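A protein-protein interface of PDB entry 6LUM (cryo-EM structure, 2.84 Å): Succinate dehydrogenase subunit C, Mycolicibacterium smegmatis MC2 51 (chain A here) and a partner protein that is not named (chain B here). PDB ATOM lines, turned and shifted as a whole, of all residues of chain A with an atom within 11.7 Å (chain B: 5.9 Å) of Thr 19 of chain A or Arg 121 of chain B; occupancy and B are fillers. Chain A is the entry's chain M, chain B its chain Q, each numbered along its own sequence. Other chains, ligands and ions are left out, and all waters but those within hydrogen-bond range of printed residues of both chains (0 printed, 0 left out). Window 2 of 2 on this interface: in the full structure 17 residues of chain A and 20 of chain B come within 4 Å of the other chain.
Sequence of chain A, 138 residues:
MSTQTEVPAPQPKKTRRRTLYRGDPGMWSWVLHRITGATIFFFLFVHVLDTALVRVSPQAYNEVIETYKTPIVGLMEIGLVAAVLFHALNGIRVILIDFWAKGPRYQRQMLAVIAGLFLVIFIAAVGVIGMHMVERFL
NH2 of Arg 88 of chain B sits close to NH2 of Arg 17 of chain A (3.1 Å). The guanidinium group (NH2) of Arg 17 of chain A is in salt-bridge range of the side-chain carboxylate (OE1) of Glu 118 of chain B (2.8 Å).
The guanidinium group (NE) of Arg 88 of chain B lies within hydrogen-bond range of the backbone carbonyl oxygen (O) of Pro 119 of chain B (2.7 Å). The side-chain amide nitrogen (ND2) of Asn 93 of chain B lies within hydrogen-bond range of the side-chain hydroxyl (OG1) of Thr 182 of chain B (2.6 Å). The backbone NH of Arg 88 of chain B sits at hydrogen-bond distance from the backbone carbonyl oxygen of Glu 118 of chain B (2.9 Å). The indole nitrogen (NE1) of Trp 188 of chain B is in hydrogen-bond range of the backbone carbonyl oxygen (O) of Thr 182 of chain B, 3.3 Å away.
OG1 of Thr 19 of chain A touches NH1 of Arg 88 of chain B, at 3.7 Å. OG1 of Thr 19 of chain A touches NH1 of Arg 121 of chain B (3.9 Å). Tyr 21 of chain A touches Asn 93 of chain B. CB of Tyr 21 of chain A touches CH2 of Trp 188 of chain B, 3.6 Å away. Trp 188 of chain B touches Met 27 of chain A.
Thr 19 of chain A touches just these residues of chain B: Arg 88 and Arg 121. Of the printed residues of chain B, Tyr 21 of chain A touches Asn 93 (3.5 Å) and Trp 188 (3.6 Å). Of the printed residues of chain B, Met 27 of chain A touches Trp 188. Trp 30 of chain A touches none of the printed residues of chain B. Of the printed residues of chain A, Glu 118 of chain B touches Arg 17 (2.8 Å). No residue of chain A comes within 4 Å of Pro 119 of chain B. Ile 120 of chain B touches none of the printed residues of chain A. Gly 122 of chain B touches none of the printed residues of chain A. Of chain A, only Tyr 21 (3.6 Å) and Met 27 (3.8 Å) come within 4 Å of Trp 188 of chain B. The nearest residue of chain B that does not touch Thr 19 of chain A is Glu 118 of chain B (4.5 Å).
Hydrophobic or aromatic side chains of chain A that line the printed part of chain B: Tyr 21 and Met 27. Of the 13 printed residues of chain B, 5 touch a printed residue of chain A. Hydrophobic or aromatic side chains of chain B that line the printed part of chain A: Trp 188. Among the printed residues, Asp or Glu carboxylates within 4 Å of a Lys or Arg side-chain nitrogen of the other chain: Arg 17 of chain A with Glu 118 of chain B (2.8 Å).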
ATOM      1  N   ARG A  16     -20.878  -1.027  21.036  1.00  0.00           N
ATOM      2  CA  ARG A  16     -21.311  -2.407  21.199  1.00  0.00           C
ATOM      3  C   ARG A  16     -20.458  -3.347  20.355  1.00  0.00           C
ATOM      4  O   ARG A  16     -20.223  -3.096  19.178  1.00  0.00           O
ATOM      5  CB  ARG A  16     -22.786  -2.551  20.827  1.00  0.00           C
ATOM      6  CG  ARG A  16     -23.747  -1.982  21.860  1.00  0.00           C
ATOM      7  CD  ARG A  16     -25.115  -1.715  21.249  1.00  0.00           C
ATOM      8  NE  ARG A  16     -26.161  -1.553  22.256  1.00  0.00           N
ATOM      9  CZ  ARG A  16     -27.422  -1.237  21.974  1.00  0.00           C
ATOM     10  NH1 ARG A  16     -27.790  -1.045  20.714  1.00  0.00           N
ATOM     11  NH2 ARG A  16     -28.315  -1.111  22.947  1.00  0.00           N
ATOM     12  N   ARG A  17     -19.996  -4.432  20.969  1.00  0.00           N
ATOM     13  CA  ARG A  17     -19.148  -5.402  20.290  1.00  0.00           C
ATOM     14  C   ARG A  17     -19.366  -6.768  20.918  1.00  0.00           C
ATOM     15  O   ARG A  17     -19.291  -6.903  22.140  1.00  0.00           O
ATOM     16  CB  ARG A  17     -17.674  -4.998  20.382  1.00  0.00           C
ATOM     17  CG  ARG A  17     -16.792  -5.586  19.297  1.00  0.00           C
ATOM     18  CD  ARG A  17     -15.328  -5.288  19.570  1.00  0.00           C
ATOM     19  NE  ARG A  17     -14.832  -6.033  20.720  1.00  0.00           N
ATOM     20  CZ  ARG A  17     -13.710  -5.748  21.372  1.00  0.00           C
ATOM     21  NH1 ARG A  17     -12.956  -4.727  20.993  1.00  0.00           N
ATOM     22  NH2 ARG A  17     -13.343  -6.487  22.405  1.00  0.00           N
ATOM     23  N   ARG A  18     -19.634  -7.771  20.088  1.00  0.00           N
ATOM     24  CA  ARG A  18     -19.911  -9.116  20.577  1.00  0.00           C
ATOM     25  C   ARG A  18     -18.597  -9.812  20.894  1.00  0.00           C
ATOM     26  O   ARG A  18     -17.804 -10.099  19.993  1.00  0.00           O
ATOM     27  CB  ARG A  18     -20.708  -9.915  19.551  1.00  0.00           C
ATOM     28  CG  ARG A  18     -20.891 -11.377  19.924  1.00  0.00           C
ATOM     29  CD  ARG A  18     -21.018 -12.251  18.689  1.00  0.00           C
ATOM     30  NE  ARG A  18     -21.640 -13.541  18.972  1.00  0.00           N
ATOM     31  CZ  ARG A  18     -20.993 -14.596  19.457  1.00  0.00           C
ATOM     32  NH1 ARG A  18     -19.697 -14.519  19.723  1.00  0.00           N
ATOM     33  NH2 ARG A  18     -21.643 -15.729  19.678  1.00  0.00           N
ATOM     34  N   THR A  19     -18.371 -10.089  22.174  1.00  0.00           N
ATOM     35  CA  THR A  19     -17.157 -10.736  22.646  1.00  0.00           C
ATOM     36  C   THR A  19     -17.517 -11.779  23.685  1.00  0.00           C
ATOM     37  O   THR A  19     -18.187 -11.464  24.671  1.00  0.00           O
ATOM     38  CB  THR A  19     -16.190  -9.719  23.259  1.00  0.00           C
ATOM     39  OG1 THR A  19     -16.876  -8.943  24.250  1.00  0.00           O
ATOM     40  CG2 THR A  19     -15.626  -8.805  22.192  1.00  0.00           C
ATOM     41  N   LEU A  20     -17.076 -13.008  23.469  1.00  0.00           N
ATOM     42  CA  LEU A  20     -17.242 -14.063  24.455  1.00  0.00           C
ATOM     43  C   LEU A  20     -16.033 -14.063  25.377  1.00  0.00           C
ATOM     44  O   LEU A  20     -14.909 -14.288  24.921  1.00  0.00           O
ATOM     45  CB  LEU A  20     -17.395 -15.418  23.777  1.00  0.00           C
ATOM     46  CG  LEU A  20     -17.640 -16.548  24.760  1.00  0.00           C
ATOM     47  CD1 LEU A  20     -19.039 -16.429  25.294  1.00  0.00           C
ATOM     48  CD2 LEU A  20     -17.429 -17.877  24.089  1.00  0.00           C
ATOM     49  N   TYR A  21     -16.257 -13.815  26.671  1.00  0.00           N
ATOM     50  CA  TYR A  21     -15.119 -13.700  27.572  1.00  0.00           C
ATOM     51  C   TYR A  21     -14.393 -15.023  27.744  1.00  0.00           C
ATOM     52  O   TYR A  21     -13.175 -15.025  27.928  1.00  0.00           O
ATOM     53  CB  TYR A  21     -15.530 -13.165  28.937  1.00  0.00           C
ATOM     54  CG  TYR A  21     -14.378 -13.209  29.911  1.00  0.00           C
ATOM     55  CD1 TYR A  21     -13.347 -12.293  29.841  1.00  0.00           C
ATOM     56  CD2 TYR A  21     -14.296 -14.198  30.864  1.00  0.00           C
ATOM     57  CE1 TYR A  21     -12.290 -12.355  30.706  1.00  0.00           C
ATOM     58  CE2 TYR A  21     -13.244 -14.262  31.721  1.00  0.00           C
ATOM     59  CZ  TYR A  21     -12.248 -13.343  31.642  1.00  0.00           C
ATOM     60  OH  TYR A  21     -11.209 -13.429  32.525  1.00  0.00           O
ATOM     61  N   ARG A  22     -15.093 -16.151  27.684  1.00  0.00           N
ATOM     62  CA  ARG A  22     -14.434 -17.451  27.758  1.00  0.00           C
ATOM     63  C   ARG A  22     -13.689 -17.605  29.084  1.00  0.00           C
ATOM     64  O   ARG A  22     -12.465 -17.677  29.139  1.00  0.00           O
ATOM     65  CB  ARG A  22     -13.491 -17.633  26.564  1.00  0.00           C
ATOM     66  CG  ARG A  22     -12.881 -18.997  26.403  1.00  0.00           C
ATOM     67  CD  ARG A  22     -12.185 -19.107  25.060  1.00  0.00           C
ATOM     68  NE  ARG A  22     -13.138 -19.166  23.956  1.00  0.00           N
ATOM     69  CZ  ARG A  22     -13.470 -18.129  23.194  1.00  0.00           C
ATOM     70  NH1 ARG A  22     -14.348 -18.280  22.213  1.00  0.00           N
ATOM     71  NH2 ARG A  22     -12.925 -16.942  23.410  1.00  0.00           N
ATOM     72  N   GLY A  23     -14.460 -17.637  30.161  1.00  0.00           N
ATOM     73  CA  GLY A  23     -13.927 -17.679  31.512  1.00  0.00           C
ATOM     74  C   GLY A  23     -14.139 -19.014  32.190  1.00  0.00           C
ATOM     75  O   GLY A  23     -13.923 -20.077  31.599  1.00  0.00           O
ATOM     76  N   MET A  27     -18.950 -19.406  35.666  1.00  0.00           N
ATOM     77  CA  MET A  27     -19.686 -18.378  34.942  1.00  0.00           C
ATOM     78  C   MET A  27     -20.861 -18.969  34.179  1.00  0.00           C
ATOM     79  O   MET A  27     -21.964 -18.411  34.179  1.00  0.00           O
ATOM     80  CB  MET A  27     -18.732 -17.657  34.000  1.00  0.00           C
ATOM     81  CG  MET A  27     -19.338 -16.570  33.173  1.00  0.00           C
ATOM     82  SD  MET A  27     -18.318 -16.283  31.729  1.00  0.00           S
ATOM     83  CE  MET A  27     -18.956 -14.717  31.204  1.00  0.00           C
ATOM     84  N   TRP A  28     -20.649 -20.111  33.535  1.00  0.00           N
ATOM     85  CA  TRP A  28     -21.727 -20.758  32.808  1.00  0.00           C
ATOM     86  C   TRP A  28     -22.745 -21.365  33.757  1.00  0.00           C
ATOM     87  O   TRP A  28     -23.949 -21.331  33.486  1.00  0.00           O
ATOM     88  CB  TRP A  28     -21.139 -21.800  31.876  1.00  0.00           C
ATOM     89  CG  TRP A  28     -20.147 -21.190  30.959  1.00  0.00           C
ATOM     90  CD1 TRP A  28     -18.824 -21.475  30.878  1.00  0.00           C
ATOM     91  CD2 TRP A  28     -20.396 -20.167  29.999  1.00  0.00           C
ATOM     92  NE1 TRP A  28     -18.232 -20.699  29.921  1.00  0.00           N
ATOM     93  CE2 TRP A  28     -19.183 -19.886  29.365  1.00  0.00           C
ATOM     94  CE3 TRP A  28     -21.535 -19.464  29.610  1.00  0.00           C
ATOM     95  CZ2 TRP A  28     -19.072 -18.934  28.368  1.00  0.00           C
ATOM     96  CZ3 TRP A  28     -21.423 -18.526  28.627  1.00  0.00           C
ATOM     97  CH2 TRP A  28     -20.205 -18.266  28.015  1.00  0.00           C
ATOM     98  N   TRP A  30     -23.485 -20.014  36.569  1.00  0.00           N
ATOM     99  CA  TRP A  30     -24.258 -18.869  37.034  1.00  0.00           C
ATOM    100  C   TRP A  30     -25.279 -18.427  36.000  1.00  0.00           C
ATOM    101  O   TRP A  30     -26.414 -18.086  36.348  1.00  0.00           O
ATOM    102  CB  TRP A  30     -23.338 -17.708  37.382  1.00  0.00           C
ATOM    103  CG  TRP A  30     -24.045 -16.411  37.388  1.00  0.00           C
ATOM    104  CD1 TRP A  30     -24.987 -16.004  38.272  1.00  0.00           C
ATOM    105  CD2 TRP A  30     -23.883 -15.343  36.457  1.00  0.00           C
ATOM    106  NE1 TRP A  30     -25.417 -14.746  37.960  1.00  0.00           N
ATOM    107  CE2 TRP A  30     -24.753 -14.319  36.844  1.00  0.00           C
ATOM    108  CE3 TRP A  30     -23.086 -15.153  35.329  1.00  0.00           C
ATOM    109  CZ2 TRP A  30     -24.845 -13.129  36.153  1.00  0.00           C
ATOM    110  CZ3 TRP A  30     -23.183 -13.973  34.648  1.00  0.00           C
ATOM    111  CH2 TRP A  30     -24.053 -12.978  35.058  1.00  0.00           C
ATOM    112  N   VAL A  31     -24.903 -18.411  34.724  1.00  0.00           N
ATOM    113  CA  VAL A  31     -25.865 -17.923  33.744  1.00  0.00           C
ATOM    114  C   VAL A  31     -26.992 -18.931  33.540  1.00  0.00           C
ATOM    115  O   VAL A  31     -28.152 -18.539  33.362  1.00  0.00           O
ATOM    116  CB  VAL A  31     -25.160 -17.540  32.432  1.00  0.00           C
ATOM    117  CG1 VAL A  31     -24.752 -18.747  31.654  1.00  0.00           C
ATOM    118  CG2 VAL A  31     -26.051 -16.651  31.609  1.00  0.00           C
ATOM    119  N   TRP B  43      -9.647  -4.662  13.787  1.00  0.00           N
ATOM    120  CA  TRP B  43      -8.857  -5.822  14.184  1.00  0.00           C
ATOM    121  C   TRP B  43      -7.699  -5.926  13.206  1.00  0.00           C
ATOM    122  O   TRP B  43      -7.809  -6.584  12.171  1.00  0.00           O
ATOM    123  CB  TRP B  43      -9.683  -7.089  14.180  1.00  0.00           C
ATOM    124  CG  TRP B  43     -10.549  -7.254  15.369  1.00  0.00           C
ATOM    125  CD1 TRP B  43     -11.761  -6.679  15.580  1.00  0.00           C
ATOM    126  CD2 TRP B  43     -10.280  -8.060  16.516  1.00  0.00           C
ATOM    127  NE1 TRP B  43     -12.267  -7.074  16.791  1.00  0.00           N
ATOM    128  CE2 TRP B  43     -11.373  -7.923  17.386  1.00  0.00           C
ATOM    129  CE3 TRP B  43      -9.218  -8.879  16.896  1.00  0.00           C
ATOM    130  CZ2 TRP B  43     -11.434  -8.574  18.609  1.00  0.00           C
ATOM    131  CZ3 TRP B  43      -9.282  -9.527  18.109  1.00  0.00           C
ATOM    132  CH2 TRP B  43     -10.380  -9.371  18.951  1.00  0.00           C
ATOM    133  N   ARG B  88      -6.916  -8.747  27.560  1.00  0.00           N
ATOM    134  CA  ARG B  88      -7.659  -9.924  27.125  1.00  0.00           C
ATOM    135  C   ARG B  88      -6.876 -10.566  25.998  1.00  0.00           C
ATOM    136  O   ARG B  88      -6.838 -10.055  24.879  1.00  0.00           O
ATOM    137  CB  ARG B  88      -9.072  -9.585  26.678  1.00  0.00           C
ATOM    138  CG  ARG B  88     -10.055  -9.377  27.781  1.00  0.00           C
ATOM    139  CD  ARG B  88     -11.410  -9.097  27.210  1.00  0.00           C
ATOM    140  NE  ARG B  88     -11.443  -7.788  26.575  1.00  0.00           N
ATOM    141  CZ  ARG B  88     -12.465  -7.320  25.874  1.00  0.00           C
ATOM    142  NH1 ARG B  88     -13.545  -8.062  25.710  1.00  0.00           N
ATOM    143  NH2 ARG B  88     -12.405  -6.111  25.341  1.00  0.00           N
ATOM    144  N   ASN B  93      -8.383 -12.543  30.646  1.00  0.00           N
ATOM    145  CA  ASN B  93      -7.446 -11.571  31.195  1.00  0.00           C
ATOM    146  C   ASN B  93      -6.159 -12.274  31.588  1.00  0.00           C
ATOM    147  O   ASN B  93      -6.189 -13.221  32.372  1.00  0.00           O
ATOM    148  CB  ASN B  93      -8.043 -10.888  32.416  1.00  0.00           C
ATOM    149  CG  ASN B  93      -9.095  -9.892  32.068  1.00  0.00           C
ATOM    150  OD1 ASN B  93      -9.577  -9.854  30.955  1.00  0.00           O
ATOM    151  ND2 ASN B  93      -9.470  -9.077  33.027  1.00  0.00           N
ATOM    152  N   GLU B 118      -6.687  -7.703  23.070  1.00  0.00           N
ATOM    153  CA  GLU B 118      -7.609  -6.583  23.169  1.00  0.00           C
ATOM    154  C   GLU B 118      -7.562  -6.046  24.587  1.00  0.00           C
ATOM    155  O   GLU B 118      -7.106  -6.739  25.495  1.00  0.00           O
ATOM    156  CB  GLU B 118      -9.028  -7.012  22.791  1.00  0.00           C
ATOM    157  CG  GLU B 118      -9.372  -8.361  23.313  1.00  0.00           C
ATOM    158  CD  GLU B 118     -10.565  -8.961  22.634  1.00  0.00           C
ATOM    159  OE1 GLU B 118     -11.216  -8.250  21.849  1.00  0.00           O
ATOM    160  OE2 GLU B 118     -10.840 -10.153  22.875  1.00  0.00           O
ATOM    161  N   PRO B 119      -8.005  -4.815  24.807  1.00  0.00           N
ATOM    162  CA  PRO B 119      -7.975  -4.262  26.162  1.00  0.00           C
ATOM    163  C   PRO B 119      -8.966  -4.951  27.080  1.00  0.00           C
ATOM    164  O   PRO B 119      -9.976  -5.502  26.644  1.00  0.00           O
ATOM    165  CB  PRO B 119      -8.349  -2.792  25.947  1.00  0.00           C
ATOM    166  CG  PRO B 119      -9.055  -2.768  24.663  1.00  0.00           C
ATOM    167  CD  PRO B 119      -8.412  -3.805  23.823  1.00  0.00           C
ATOM    168  N   ILE B 120      -8.672  -4.901  28.379  1.00  0.00           N
ATOM    169  CA  ILE B 120      -9.532  -5.558  29.350  1.00  0.00           C
ATOM    170  C   ILE B 120     -10.884  -4.861  29.390  1.00  0.00           C
ATOM    171  O   ILE B 120     -11.002  -3.660  29.130  1.00  0.00           O
ATOM    172  CB  ILE B 120      -8.882  -5.595  30.744  1.00  0.00           C
ATOM    173  CG1 ILE B 120      -8.519  -4.200  31.229  1.00  0.00           C
ATOM    174  CG2 ILE B 120      -7.656  -6.463  30.737  1.00  0.00           C
ATOM    175  CD1 ILE B 120      -7.855  -4.203  32.571  1.00  0.00           C
ATOM    176  N   ARG B 121     -11.915  -5.625  29.723  1.00  0.00           N
ATOM    177  CA  ARG B 121     -13.287  -5.163  29.644  1.00  0.00           C
ATOM    178  C   ARG B 121     -13.606  -4.235  30.811  1.00  0.00           C
ATOM    179  O   ARG B 121     -12.771  -3.971  31.673  1.00  0.00           O
ATOM    180  CB  ARG B 121     -14.224  -6.362  29.610  1.00  0.00           C
ATOM    181  CG  ARG B 121     -15.536  -6.087  28.945  1.00  0.00           C
ATOM    182  CD  ARG B 121     -16.262  -7.349  28.593  1.00  0.00           C
ATOM    183  NE  ARG B 121     -17.696  -7.136  28.663  1.00  0.00           N
ATOM    184  CZ  ARG B 121     -18.597  -8.043  28.329  1.00  0.00           C
ATOM    185  NH1 ARG B 121     -18.205  -9.229  27.895  1.00  0.00           N
ATOM    186  NH2 ARG B 121     -19.884  -7.762  28.432  1.00  0.00           N
ATOM    187  N   GLY B 122     -14.823  -3.709  30.828  1.00  0.00           N
ATOM    188  CA  GLY B 122     -15.302  -2.944  31.960  1.00  0.00           C
ATOM    189  C   GLY B 122     -14.867  -1.495  32.004  1.00  0.00           C
ATOM    190  O   GLY B 122     -15.654  -0.621  32.373  1.00  0.00           O
ATOM    191  N   LEU B 123     -13.645  -1.229  31.648  1.00  0.00           N
ATOM    192  CA  LEU B 123     -13.067   0.096  31.774  1.00  0.00           C
ATOM    193  C   LEU B 123     -13.039   0.807  30.428  1.00  0.00           C
ATOM    194  O   LEU B 123     -12.944   0.162  29.381  1.00  0.00           O
ATOM    195  CB  LEU B 123     -11.644   0.010  32.324  1.00  0.00           C
ATOM    196  CG  LEU B 123     -11.496  -0.384  33.784  1.00  0.00           C
ATOM    197  CD1 LEU B 123     -10.130  -0.955  34.015  1.00  0.00           C
ATOM    198  CD2 LEU B 123     -11.708   0.816  34.652  1.00  0.00           C
ATOM    199  N   VAL B 131      -6.365   1.141  28.941  1.00  0.00           N
ATOM    200  CA  VAL B 131      -7.659   1.491  29.495  1.00  0.00           C
ATOM    201  C   VAL B 131      -7.474   2.574  30.546  1.00  0.00           C
ATOM    202  O   VAL B 131      -6.376   2.811  31.050  1.00  0.00           O
ATOM    203  CB  VAL B 131      -8.381   0.265  30.080  1.00  0.00           C
ATOM    204  CG1 VAL B 131      -8.781  -0.669  28.970  1.00  0.00           C
ATOM    205  CG2 VAL B 131      -7.494  -0.452  31.048  1.00  0.00           C
ATOM    206  N   THR B 182     -12.072  -6.702  36.120  1.00  0.00           N
ATOM    207  CA  THR B 182     -12.531  -6.606  34.748  1.00  0.00           C
ATOM    208  C   THR B 182     -12.899  -7.951  34.156  1.00  0.00           C
ATOM    209  O   THR B 182     -13.048  -8.054  32.939  1.00  0.00           O
ATOM    210  CB  THR B 182     -11.470  -5.943  33.889  1.00  0.00           C
ATOM    211  OG1 THR B 182     -10.278  -6.725  33.928  1.00  0.00           O
ATOM    212  CG2 THR B 182     -11.177  -4.568  34.409  1.00  0.00           C
ATOM    213  N   TYR B 187     -19.551  -6.687  37.507  1.00  0.00           N
ATOM    214  CA  TYR B 187     -18.911  -5.421  37.189  1.00  0.00           C
ATOM    215  C   TYR B 187     -19.283  -4.967  35.792  1.00  0.00           C
ATOM    216  O   TYR B 187     -19.421  -3.770  35.538  1.00  0.00           O
ATOM    217  CB  TYR B 187     -17.399  -5.561  37.325  1.00  0.00           C
ATOM    218  CG  TYR B 187     -16.648  -4.264  37.265  1.00  0.00           C
ATOM    219  CD1 TYR B 187     -16.655  -3.392  38.331  1.00  0.00           C
ATOM    220  CD2 TYR B 187     -15.922  -3.918  36.141  1.00  0.00           C
ATOM    221  CE1 TYR B 187     -15.975  -2.215  38.277  1.00  0.00           C
ATOM    222  CE2 TYR B 187     -15.237  -2.742  36.079  1.00  0.00           C
ATOM    223  CZ  TYR B 187     -15.265  -1.894  37.148  1.00  0.00           C
ATOM    224  OH  TYR B 187     -14.579  -0.709  37.091  1.00  0.00           O
ATOM    225  N   TRP B 188     -19.451  -5.915  34.877  1.00  0.00           N
ATOM    226  CA  TRP B 188     -19.929  -5.585  33.541  1.00  0.00           C
ATOM    227  C   TRP B 188     -21.361  -5.068  33.554  1.00  0.00           C
ATOM    228  O   TRP B 188     -21.732  -4.274  32.687  1.00  0.00           O
ATOM    229  CB  TRP B 188     -19.842  -6.808  32.643  1.00  0.00           C
ATOM    230  CG  TRP B 188     -18.490  -7.382  32.545  1.00  0.00           C
ATOM    231  CD1 TRP B 188     -17.325  -6.749  32.783  1.00  0.00           C
ATOM    232  CD2 TRP B 188     -18.157  -8.715  32.163  1.00  0.00           C
ATOM    233  NE1 TRP B 188     -16.280  -7.598  32.575  1.00  0.00           N
ATOM    234  CE2 TRP B 188     -16.767  -8.816  32.192  1.00  0.00           C
ATOM    235  CE3 TRP B 188     -18.903  -9.832  31.799  1.00  0.00           C
ATOM    236  CZ2 TRP B 188     -16.103  -9.988  31.874  1.00  0.00           C
ATOM    237  CZ3 TRP B 188     -18.243 -10.989  31.489  1.00  0.00           C
ATOM    238  CH2 TRP B 188     -16.860 -11.061  31.529  1.00  0.00           C
